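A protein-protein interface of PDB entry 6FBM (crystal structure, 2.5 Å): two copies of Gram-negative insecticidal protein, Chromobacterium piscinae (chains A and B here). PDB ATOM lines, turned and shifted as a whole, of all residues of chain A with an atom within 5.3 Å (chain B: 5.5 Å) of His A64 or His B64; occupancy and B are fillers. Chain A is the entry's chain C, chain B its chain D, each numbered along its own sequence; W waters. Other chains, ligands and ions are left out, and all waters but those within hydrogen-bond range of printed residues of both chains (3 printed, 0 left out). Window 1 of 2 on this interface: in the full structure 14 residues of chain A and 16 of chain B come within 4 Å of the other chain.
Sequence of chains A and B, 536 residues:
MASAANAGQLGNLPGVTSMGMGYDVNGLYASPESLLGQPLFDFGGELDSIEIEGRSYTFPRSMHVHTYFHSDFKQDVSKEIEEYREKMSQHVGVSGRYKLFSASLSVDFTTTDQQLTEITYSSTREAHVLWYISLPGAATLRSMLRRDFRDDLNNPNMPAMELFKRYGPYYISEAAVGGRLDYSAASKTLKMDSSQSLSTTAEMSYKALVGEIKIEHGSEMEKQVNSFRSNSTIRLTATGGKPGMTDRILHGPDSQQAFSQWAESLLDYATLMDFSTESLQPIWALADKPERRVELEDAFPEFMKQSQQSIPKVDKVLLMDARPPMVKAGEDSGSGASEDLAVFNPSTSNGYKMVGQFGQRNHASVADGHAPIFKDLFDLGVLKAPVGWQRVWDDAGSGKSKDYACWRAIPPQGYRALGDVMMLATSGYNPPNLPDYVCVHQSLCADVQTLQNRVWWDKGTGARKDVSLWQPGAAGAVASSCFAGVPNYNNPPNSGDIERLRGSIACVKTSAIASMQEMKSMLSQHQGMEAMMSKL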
ATOM      1  N   PHE A  59      37.787 -14.652  14.571  1.00  0.00           N
ATOM      2  CA  PHE A  59      36.801 -13.841  15.277  1.00  0.00           C
ATOM      3  C   PHE A  59      35.759 -14.799  15.839  1.00  0.00           C
ATOM      4  O   PHE A  59      35.694 -15.939  15.403  1.00  0.00           O
ATOM      5  CB  PHE A  59      36.155 -12.823  14.339  1.00  0.00           C
ATOM      6  CG  PHE A  59      35.498 -13.450  13.155  1.00  0.00           C
ATOM      7  CD1 PHE A  59      36.229 -13.775  12.030  1.00  0.00           C
ATOM      8  CD2 PHE A  59      34.137 -13.720  13.166  1.00  0.00           C
ATOM      9  CE1 PHE A  59      35.632 -14.355  10.924  1.00  0.00           C
ATOM     10  CE2 PHE A  59      33.509 -14.313  12.075  1.00  0.00           C
ATOM     11  CZ  PHE A  59      34.264 -14.628  10.936  1.00  0.00           C
ATOM     12  N   PRO A  60      34.952 -14.360  16.813  1.00  0.00           N
ATOM     13  CA  PRO A  60      33.932 -15.263  17.373  1.00  0.00           C
ATOM     14  C   PRO A  60      32.866 -15.672  16.365  1.00  0.00           C
ATOM     15  O   PRO A  60      32.392 -14.818  15.602  1.00  0.00           O
ATOM     16  CB  PRO A  60      33.330 -14.430  18.511  1.00  0.00           C
ATOM     17  CG  PRO A  60      34.472 -13.588  18.929  1.00  0.00           C
ATOM     18  CD  PRO A  60      35.008 -13.140  17.593  1.00  0.00           C
ATOM     19  N   ARG A  61      32.528 -16.950  16.355  1.00  0.00           N
ATOM     20  CA  ARG A  61      31.464 -17.523  15.494  1.00  0.00           C
ATOM     21  C   ARG A  61      30.158 -16.739  15.558  1.00  0.00           C
ATOM     22  O   ARG A  61      29.456 -16.604  14.603  1.00  0.00           O
ATOM     23  CB  ARG A  61      31.141 -18.969  15.903  1.00  0.00           C
ATOM     24  CG  ARG A  61      31.644 -19.977  14.902  1.00  0.00           C
ATOM     25  CD  ARG A  61      31.611 -21.421  15.380  1.00  0.00           C
ATOM     26  NE  ARG A  61      32.764 -22.152  14.844  1.00  0.00           N
ATOM     27  CZ  ARG A  61      32.936 -22.476  13.549  1.00  0.00           C
ATOM     28  NH1 ARG A  61      32.071 -22.068  12.596  1.00  0.00           N
ATOM     29  NH2 ARG A  61      34.043 -23.130  13.168  1.00  0.00           N
ATOM     30  N   SER A  62      29.851 -16.258  16.750  1.00  0.00           N
ATOM     31  CA  SER A  62      28.657 -15.493  16.992  1.00  0.00           C
ATOM     32  C   SER A  62      28.631 -14.128  16.304  1.00  0.00           C
ATOM     33  O   SER A  62      27.546 -13.534  16.220  1.00  0.00           O
ATOM     34  CB  SER A  62      28.432 -15.345  18.495  1.00  0.00           C
ATOM     35  OG  SER A  62      29.555 -14.778  19.125  1.00  0.00           O
ATOM     36  N   MET A  63      29.761 -13.623  15.812  1.00  0.00           N
ATOM     37  CA  MET A  63      29.755 -12.367  15.072  1.00  0.00           C
ATOM     38  C   MET A  63      29.742 -12.693  13.607  1.00  0.00           C
ATOM     39  O   MET A  63      30.129 -13.790  13.198  1.00  0.00           O
ATOM     40  CB  MET A  63      30.981 -11.500  15.380  1.00  0.00           C
ATOM     41  CG  MET A  63      31.167 -11.238  16.841  1.00  0.00           C
ATOM     42  SD  MET A  63      32.538 -10.106  17.199  1.00  0.00           S
ATOM     43  CE  MET A  63      32.543 -10.226  19.036  1.00  0.00           C
ATOM     44  N   HIS A  64      29.298 -11.713  12.836  1.00  0.00           N
ATOM     45  CA  HIS A  64      29.284 -11.794  11.386  1.00  0.00           C
ATOM     46  C   HIS A  64      30.210 -10.737  10.838  1.00  0.00           C
ATOM     47  O   HIS A  64      30.215  -9.604  11.322  1.00  0.00           O
ATOM     48  CB  HIS A  64      27.877 -11.540  10.840  1.00  0.00           C
ATOM     49  CG  HIS A  64      26.964 -12.716  10.933  1.00  0.00           C
ATOM     50  ND1 HIS A  64      25.732 -12.746  10.298  1.00  0.00           N
ATOM     51  CD2 HIS A  64      27.123 -13.924  11.514  1.00  0.00           C
ATOM     52  CE1 HIS A  64      25.168 -13.920  10.516  1.00  0.00           C
ATOM     53  NE2 HIS A  64      25.996 -14.661  11.230  1.00  0.00           N
ATOM     54  N   VAL A  65      30.938 -11.110   9.787  1.00  0.00           N
ATOM     55  CA  VAL A  65      31.846 -10.225   9.127  1.00  0.00           C
ATOM     56  C   VAL A  65      31.408 -10.094   7.694  1.00  0.00           C
ATOM     57  O   VAL A  65      31.203 -11.085   7.017  1.00  0.00           O
ATOM     58  CB  VAL A  65      33.275 -10.775   9.196  1.00  0.00           C
ATOM     59  CG1 VAL A  65      34.228  -9.895   8.404  1.00  0.00           C
ATOM     60  CG2 VAL A  65      33.737 -10.940  10.657  1.00  0.00           C
ATOM     61  N   HIS A  66      31.338  -8.858   7.230  1.00  0.00           N
ATOM     62  CA  HIS A  66      31.116  -8.507   5.832  1.00  0.00           C
ATOM     63  C   HIS A  66      32.280  -7.658   5.346  1.00  0.00           C
ATOM     64  O   HIS A  66      32.425  -6.507   5.744  1.00  0.00           O
ATOM     65  CB  HIS A  66      29.803  -7.725   5.708  1.00  0.00           C
ATOM     66  CG  HIS A  66      28.597  -8.592   5.748  1.00  0.00           C
ATOM     67  ND1 HIS A  66      27.967  -8.938   6.930  1.00  0.00           N
ATOM     68  CD2 HIS A  66      27.923  -9.214   4.751  1.00  0.00           C
ATOM     69  CE1 HIS A  66      26.930  -9.715   6.647  1.00  0.00           C
ATOM     70  NE2 HIS A  66      26.886  -9.901   5.338  1.00  0.00           N
ATOM     71  N   TYR A 132      32.752  -4.772   8.008  1.00  0.00           N
ATOM     72  CA  TYR A 132      31.793  -4.517   9.050  1.00  0.00           C
ATOM     73  C   TYR A 132      31.754  -5.757   9.916  1.00  0.00           C
ATOM     74  O   TYR A 132      31.939  -6.884   9.411  1.00  0.00           O
ATOM     75  CB  TYR A 132      30.396  -4.268   8.472  1.00  0.00           C
ATOM     76  CG  TYR A 132      30.295  -3.173   7.444  1.00  0.00           C
ATOM     77  CD1 TYR A 132      30.134  -1.835   7.832  1.00  0.00           C
ATOM     78  CD2 TYR A 132      30.330  -3.463   6.076  1.00  0.00           C
ATOM     79  CE1 TYR A 132      30.028  -0.804   6.908  1.00  0.00           C
ATOM     80  CE2 TYR A 132      30.268  -2.420   5.103  1.00  0.00           C
ATOM     81  CZ  TYR A 132      30.090  -1.103   5.534  1.00  0.00           C
ATOM     82  OH  TYR A 132      29.980  -0.100   4.607  1.00  0.00           O
ATOM     83  N   ILE A 133      31.598  -5.564  11.220  1.00  0.00           N
ATOM     84  CA  ILE A 133      31.378  -6.657  12.129  1.00  0.00           C
ATOM     85  C   ILE A 133      30.036  -6.365  12.748  1.00  0.00           C
ATOM     86  O   ILE A 133      29.721  -5.194  13.024  1.00  0.00           O
ATOM     87  CB  ILE A 133      32.442  -6.757  13.252  1.00  0.00           C
ATOM     88  CG1 ILE A 133      33.861  -6.537  12.685  1.00  0.00           C
ATOM     89  CG2 ILE A 133      32.311  -8.115  13.948  1.00  0.00           C
ATOM     90  CD1 ILE A 133      34.924  -6.504  13.732  1.00  0.00           C
ATOM     91  N   SER A 134      29.226  -7.409  12.942  1.00  0.00           N
ATOM     92  CA  SER A 134      27.880  -7.226  13.522  1.00  0.00           C
ATOM     93  C   SER A 134      27.564  -8.352  14.466  1.00  0.00           C
ATOM     94  O   SER A 134      28.056  -9.453  14.287  1.00  0.00           O
ATOM     95  CB  SER A 134      26.817  -7.119  12.445  1.00  0.00           C
ATOM     96  OG  SER A 134      26.835  -8.279  11.636  1.00  0.00           O
ATOM     97  N   LEU A 135      26.801  -8.042  15.499  1.00  0.00           N
ATOM     98  CA  LEU A 135      26.397  -8.993  16.515  1.00  0.00           C
ATOM     99  C   LEU A 135      24.980  -9.519  16.268  1.00  0.00           C
ATOM    100  O   LEU A 135      24.244  -8.963  15.440  1.00  0.00           O
ATOM    101  CB  LEU A 135      26.401  -8.277  17.875  1.00  0.00           C
ATOM    102  CG  LEU A 135      27.746  -7.755  18.349  1.00  0.00           C
ATOM    103  CD1 LEU A 135      27.564  -7.196  19.755  1.00  0.00           C
ATOM    104  CD2 LEU A 135      28.777  -8.839  18.364  1.00  0.00           C
ATOM    105  N   PRO A 136      24.560 -10.540  17.036  1.00  0.00           N
ATOM    106  CA  PRO A 136      23.154 -10.891  17.097  1.00  0.00           C
ATOM    107  C   PRO A 136      22.286  -9.764  17.634  1.00  0.00           C
ATOM    108  O   PRO A 136      22.784  -8.803  18.250  1.00  0.00           O
ATOM    109  CB  PRO A 136      23.116 -12.075  18.058  1.00  0.00           C
ATOM    110  CG  PRO A 136      24.474 -12.655  18.042  1.00  0.00           C
ATOM    111  CD  PRO A 136      25.362 -11.451  17.869  1.00  0.00           C
ATOM    112  N   PHE B  59      17.491 -21.489  16.126  1.00  0.00           N
ATOM    113  CA  PHE B  59      17.984 -21.279  14.772  1.00  0.00           C
ATOM    114  C   PHE B  59      19.483 -21.478  14.839  1.00  0.00           C
ATOM    115  O   PHE B  59      20.058 -21.442  15.933  1.00  0.00           O
ATOM    116  CB  PHE B  59      17.633 -19.873  14.292  1.00  0.00           C
ATOM    117  CG  PHE B  59      18.139 -18.795  15.163  1.00  0.00           C
ATOM    118  CD1 PHE B  59      17.419 -18.401  16.288  1.00  0.00           C
ATOM    119  CD2 PHE B  59      19.342 -18.168  14.881  1.00  0.00           C
ATOM    120  CE1 PHE B  59      17.888 -17.392  17.127  1.00  0.00           C
ATOM    121  CE2 PHE B  59      19.810 -17.155  15.708  1.00  0.00           C
ATOM    122  CZ  PHE B  59      19.085 -16.776  16.845  1.00  0.00           C
ATOM    123  N   PRO B  60      20.133 -21.703  13.692  1.00  0.00           N
ATOM    124  CA  PRO B  60      21.582 -21.891  13.724  1.00  0.00           C
ATOM    125  C   PRO B  60      22.352 -20.652  14.206  1.00  0.00           C
ATOM    126  O   PRO B  60      22.037 -19.543  13.831  1.00  0.00           O
ATOM    127  CB  PRO B  60      21.900 -22.227  12.279  1.00  0.00           C
ATOM    128  CG  PRO B  60      20.643 -22.736  11.695  1.00  0.00           C
ATOM    129  CD  PRO B  60      19.602 -21.882  12.331  1.00  0.00           C
ATOM    130  N   ARG B  61      23.333 -20.870  15.064  1.00  0.00           N
ATOM    131  CA  ARG B  61      24.209 -19.805  15.576  1.00  0.00           C
ATOM    132  C   ARG B  61      24.891 -19.047  14.485  1.00  0.00           C
ATOM    133  O   ARG B  61      25.147 -17.877  14.677  1.00  0.00           O
ATOM    134  CB  ARG B  61      25.212 -20.349  16.633  1.00  0.00           C
ATOM    135  CG  ARG B  61      26.563 -19.619  16.868  1.00  0.00           C
ATOM    136  CD  ARG B  61      26.775 -18.910  18.231  1.00  0.00           C
ATOM    137  NE  ARG B  61      26.881 -19.851  19.350  1.00  0.00           N
ATOM    138  CZ  ARG B  61      26.639 -19.558  20.634  1.00  0.00           C
ATOM    139  NH1 ARG B  61      26.227 -18.336  21.008  1.00  0.00           N
ATOM    140  NH2 ARG B  61      26.791 -20.515  21.560  1.00  0.00           N
ATOM    141  N   SER B  62      25.144 -19.662  13.342  1.00  0.00           N
ATOM    142  CA  SER B  62      25.681 -18.958  12.198  1.00  0.00           C
ATOM    143  C   SER B  62      24.760 -17.900  11.594  1.00  0.00           C
ATOM    144  O   SER B  62      25.219 -17.072  10.839  1.00  0.00           O
ATOM    145  CB  SER B  62      26.127 -19.972  11.137  1.00  0.00           C
ATOM    146  OG  SER B  62      25.094 -20.820  10.763  1.00  0.00           O
ATOM    147  N   MET B  63      23.476 -17.907  11.910  1.00  0.00           N
ATOM    148  CA  MET B  63      22.561 -16.840  11.449  1.00  0.00           C
ATOM    149  C   MET B  63      22.407 -15.853  12.568  1.00  0.00           C
ATOM    150  O   MET B  63      22.612 -16.190  13.722  1.00  0.00           O
ATOM    151  CB  MET B  63      21.197 -17.369  11.065  1.00  0.00           C
ATOM    152  CG  MET B  63      21.234 -18.529  10.105  1.00  0.00           C
ATOM    153  SD  MET B  63      19.616 -19.095   9.538  1.00  0.00           S
ATOM    154  CE  MET B  63      20.138 -20.462   8.541  1.00  0.00           C
ATOM    155  N   HIS B  64      22.026 -14.647  12.213  1.00  0.00           N
ATOM    156  CA  HIS B  64      21.683 -13.600  13.159  1.00  0.00           C
ATOM    157  C   HIS B  64      20.220 -13.267  13.016  1.00  0.00           C
ATOM    158  O   HIS B  64      19.721 -13.172  11.895  1.00  0.00           O
ATOM    159  CB  HIS B  64      22.508 -12.336  12.895  1.00  0.00           C
ATOM    160  CG  HIS B  64      23.910 -12.413  13.437  1.00  0.00           C
ATOM    161  ND1 HIS B  64      24.809 -11.375  13.338  1.00  0.00           N
ATOM    162  CD2 HIS B  64      24.565 -13.422  14.066  1.00  0.00           C
ATOM    163  CE1 HIS B  64      25.953 -11.748  13.888  1.00  0.00           C
ATOM    164  NE2 HIS B  64      25.835 -12.981  14.331  1.00  0.00           N
ATOM    165  N   VAL B  65      19.558 -13.082  14.152  1.00  0.00           N
ATOM    166  CA  VAL B  65      18.174 -12.755  14.197  1.00  0.00           C
ATOM    167  C   VAL B  65      18.029 -11.424  14.888  1.00  0.00           C
ATOM    168  O   VAL B  65      18.564 -11.208  15.973  1.00  0.00           O
ATOM    169  CB  VAL B  65      17.391 -13.841  14.944  1.00  0.00           C
ATOM    170  CG1 VAL B  65      15.955 -13.428  15.173  1.00  0.00           C
ATOM    171  CG2 VAL B  65      17.341 -15.075  14.053  1.00  0.00           C
ATOM    172  N   HIS B  66      17.268 -10.555  14.252  1.00  0.00           N
ATOM    173  CA  HIS B  66      16.917  -9.240  14.756  1.00  0.00           C
ATOM    174  C   HIS B  66      15.396  -9.151  14.809  1.00  0.00           C
ATOM    175  O   HIS B  66      14.734  -9.114  13.773  1.00  0.00           O
ATOM    176  CB  HIS B  66      17.483  -8.180  13.801  1.00  0.00           C
ATOM    177  CG  HIS B  66      18.932  -7.919  14.020  1.00  0.00           C
ATOM    178  ND1 HIS B  66      19.931  -8.644  13.400  1.00  0.00           N
ATOM    179  CD2 HIS B  66      19.550  -7.019  14.820  1.00  0.00           C
ATOM    180  CE1 HIS B  66      21.103  -8.235  13.854  1.00  0.00           C
ATOM    181  NE2 HIS B  66      20.903  -7.233  14.700  1.00  0.00           N
ATOM    182  N   TYR B 132      14.067 -10.334  11.279  1.00  0.00           N
ATOM    183  CA  TYR B 132      14.943 -10.439  10.114  1.00  0.00           C
ATOM    184  C   TYR B 132      15.935 -11.541  10.488  1.00  0.00           C
ATOM    185  O   TYR B 132      16.301 -11.679  11.640  1.00  0.00           O
ATOM    186  CB  TYR B 132      15.646  -9.122   9.802  1.00  0.00           C
ATOM    187  CG  TYR B 132      15.121  -8.318   8.603  1.00  0.00           C
ATOM    188  CD1 TYR B 132      14.072  -7.430   8.724  1.00  0.00           C
ATOM    189  CD2 TYR B 132      15.726  -8.454   7.350  1.00  0.00           C
ATOM    190  CE1 TYR B 132      13.645  -6.639   7.670  1.00  0.00           C
ATOM    191  CE2 TYR B 132      15.286  -7.694   6.234  1.00  0.00           C
ATOM    192  CZ  TYR B 132      14.247  -6.779   6.403  1.00  0.00           C
ATOM    193  OH  TYR B 132      13.796  -6.017   5.331  1.00  0.00           O
ATOM    194  N   ILE B 133      16.297 -12.346   9.515  1.00  0.00           N
ATOM    195  CA  ILE B 133      17.335 -13.345   9.665  1.00  0.00           C
ATOM    196  C   ILE B 133      18.390 -12.941   8.644  1.00  0.00           C
ATOM    197  O   ILE B 133      18.040 -12.531   7.545  1.00  0.00           O
ATOM    198  CB  ILE B 133      16.879 -14.778   9.393  1.00  0.00           C
ATOM    199  CG1 ILE B 133      15.539 -15.075  10.089  1.00  0.00           C
ATOM    200  CG2 ILE B 133      17.926 -15.730   9.912  1.00  0.00           C
ATOM    201  CD1 ILE B 133      14.934 -16.445   9.753  1.00  0.00           C
ATOM    202  N   SER B 134      19.664 -13.027   9.018  1.00  0.00           N
ATOM    203  CA  SER B 134      20.754 -12.671   8.116  1.00  0.00           C
ATOM    204  C   SER B 134      21.910 -13.617   8.248  1.00  0.00           C
ATOM    205  O   SER B 134      22.122 -14.171   9.300  1.00  0.00           O
ATOM    206  CB  SER B 134      21.221 -11.238   8.372  1.00  0.00           C
ATOM    207  OG  SER B 134      21.653 -11.074   9.686  1.00  0.00           O
ATOM    208  N   LEU B 135      22.580 -13.859   7.139  1.00  0.00           N
ATOM    209  CA  LEU B 135      23.711 -14.788   7.053  1.00  0.00           C
ATOM    210  C   LEU B 135      25.037 -14.029   7.077  1.00  0.00           C
ATOM    211  O   LEU B 135      25.051 -12.807   6.845  1.00  0.00           O
ATOM    212  CB  LEU B 135      23.645 -15.571   5.737  1.00  0.00           C
ATOM    213  CG  LEU B 135      22.401 -16.421   5.537  1.00  0.00           C
ATOM    214  CD1 LEU B 135      22.525 -17.158   4.228  1.00  0.00           C
ATOM    215  CD2 LEU B 135      22.165 -17.391   6.700  1.00  0.00           C
ATOM    216  N   PRO B 136      26.135 -14.749   7.313  1.00  0.00           N
ATOM    217  CA  PRO B 136      27.454 -14.168   7.137  1.00  0.00           C
ATOM    218  C   PRO B 136      27.720 -13.739   5.684  1.00  0.00           C
ATOM    219  O   PRO B 136      26.978 -14.140   4.752  1.00  0.00           O
ATOM    220  CB  PRO B 136      28.419 -15.325   7.514  1.00  0.00           C
ATOM    221  CG  PRO B 136      27.609 -16.249   8.322  1.00  0.00           C
ATOM    222  CD  PRO B 136      26.245 -16.162   7.733  1.00  0.00           C
HETATM  223  O   HOH W   1      23.549 -10.551   5.135  1.00  0.00           O
HETATM  224  O   HOH W   2      23.936  -8.986  11.980  1.00  0.00           O
HETATM  225  O   HOH W   3      24.608 -10.235   9.131  1.00  0.00           O
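NE2 of His B64 is in hydrogen-bond range of O of Ser A62, at 2.6 Å.
NE2 of His A64 lies within hydrogen-bond range of O of Ser B62.
ND1 of His A64 is in hydrogen-bond range of ND1 of His B64.
The backbone carbonyl oxygen (O) of Leu A135 sits at hydrogen-bond distance from a ring nitrogen (ND1) of His B64, 3.2 Å away.
The backbone NH (N) of Ser A134 is in hydrogen-bond range of the backbone carbonyl oxygen (O) of His A64, at 2.9 Å.
The backbone carbonyl oxygen (O) of His A66 is in hydrogen-bond range of the backbone NH (N) of Tyr A132, at 2.9 Å.
O of His B64 lies within hydrogen-bond range of N of Ser B134 (2.9 Å).
The backbone carbonyl oxygen (O) of His B66 sits at hydrogen-bond distance from the backbone NH (N) of Tyr B132, at 2.9 Å.
C of Met A63 touches CE1 of His B64 (3.9 Å).
His A64 touches Met B63 (CE1 to C, 3.9 Å).
Ser B134 touches His A64 (O to CE1, 3.3 Å).
CE1 of His A64 touches C of Leu B135 (3.4 Å).
Pro B136 touches His A64.
O of Leu B135 touches CE1 of His A66, 3.6 Å away.
His A66 touches Pro B136.
Ser A134 touches His B64.
Leu A135 touches His B66.
Pro A136 touches His B64.
Of the printed residues of chain B, Met A63 touches His B64 (3.9 Å).
His A64 touches just these residues of chain B: Ser B62 (2.6 Å), Met B63 (3.9 Å), His B64 (3.2 Å), Ser B134 (3.3 Å), Leu B135 (3.4 Å) and Pro B136 (3.4 Å).
Of the printed residues of chain B, Ser A134 touches His B64 (3.1 Å).
Of the printed residues of chain B, Pro A136 touches His B64 (3.6 Å).
Printed residues of chain A within 4 Å of Arg B61: Ser A62.
Of chain A, only Ser A62 (2.6 Å), Met A63 (3.9 Å), His A64 (3.2 Å), Ser A134 (3.1 Å), Leu A135 (3.2 Å) and Pro A136 (3.6 Å) come within 4 Å of His B64.
Of the printed residues of chain A, Leu B135 touches His A64 and His A66.
The nearest residue of chain B that does not touch His A64 is Arg B61 (4.8 Å).
The nearest printed residue of chain B that does not touch Met A63 is Pro B136 (6.0 Å).
Of the 13 printed residues of chain B, 8 touch a printed residue of chain A.
Printed residues of chain B that touch a printed residue of chain A: Arg B61, Ser B62, Met B63, His B64, His B66, Ser B134, Leu B135 and Pro B136.
Hydrophobic or aromatic side chains of chain B that line the printed part of chain A: His B64, His B66 and Pro B136.
Hydrophobic or aromatic side chains of chain A within 4 Å of the printed part of chain B: His A64, His A66 and Pro A136.
Among the printed residues, 15 pairs touch across the chains.
Among the printed residues, no Asp or Glu carboxylate lies within 4 Å of a Lys or Arg side-chain nitrogen of the other chain.
Ser A62 touches His B64, and with the chains exchanged His A64 touches Ser B62.
His A64 touches its own counterpart, His B64.
His A64 touches Leu B135, and with the chains exchanged Leu A135 touches His B64.
His A66 touches Leu B135, and with the chains exchanged Leu A135 touches His B66.
Positions printed for both chains: 59, 60, 61, 62, 63, 64, 65, 66, 132, 133, 134, 135 and 136.
Water W2 lies within hydrogen-bond range of a ring nitrogen (ND1) of His B64 (2.9 Å), the side-chain hydroxyl of Ser A134 (3.0 Å) and the backbone carbonyl oxygen of Leu A135 (3.5 Å).
Water W3 lies within hydrogen-bond range of ND1 of His A64 (3.0 Å), OG of Ser B134 (3.1 Å) and O of Leu B135 (3.5 Å).
Water W1 lies within hydrogen-bond range of the backbone carbonyl oxygen (O) of Leu B135 (3.2 Å) and a ring nitrogen (NE2) of His A66 (3.4 Å).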
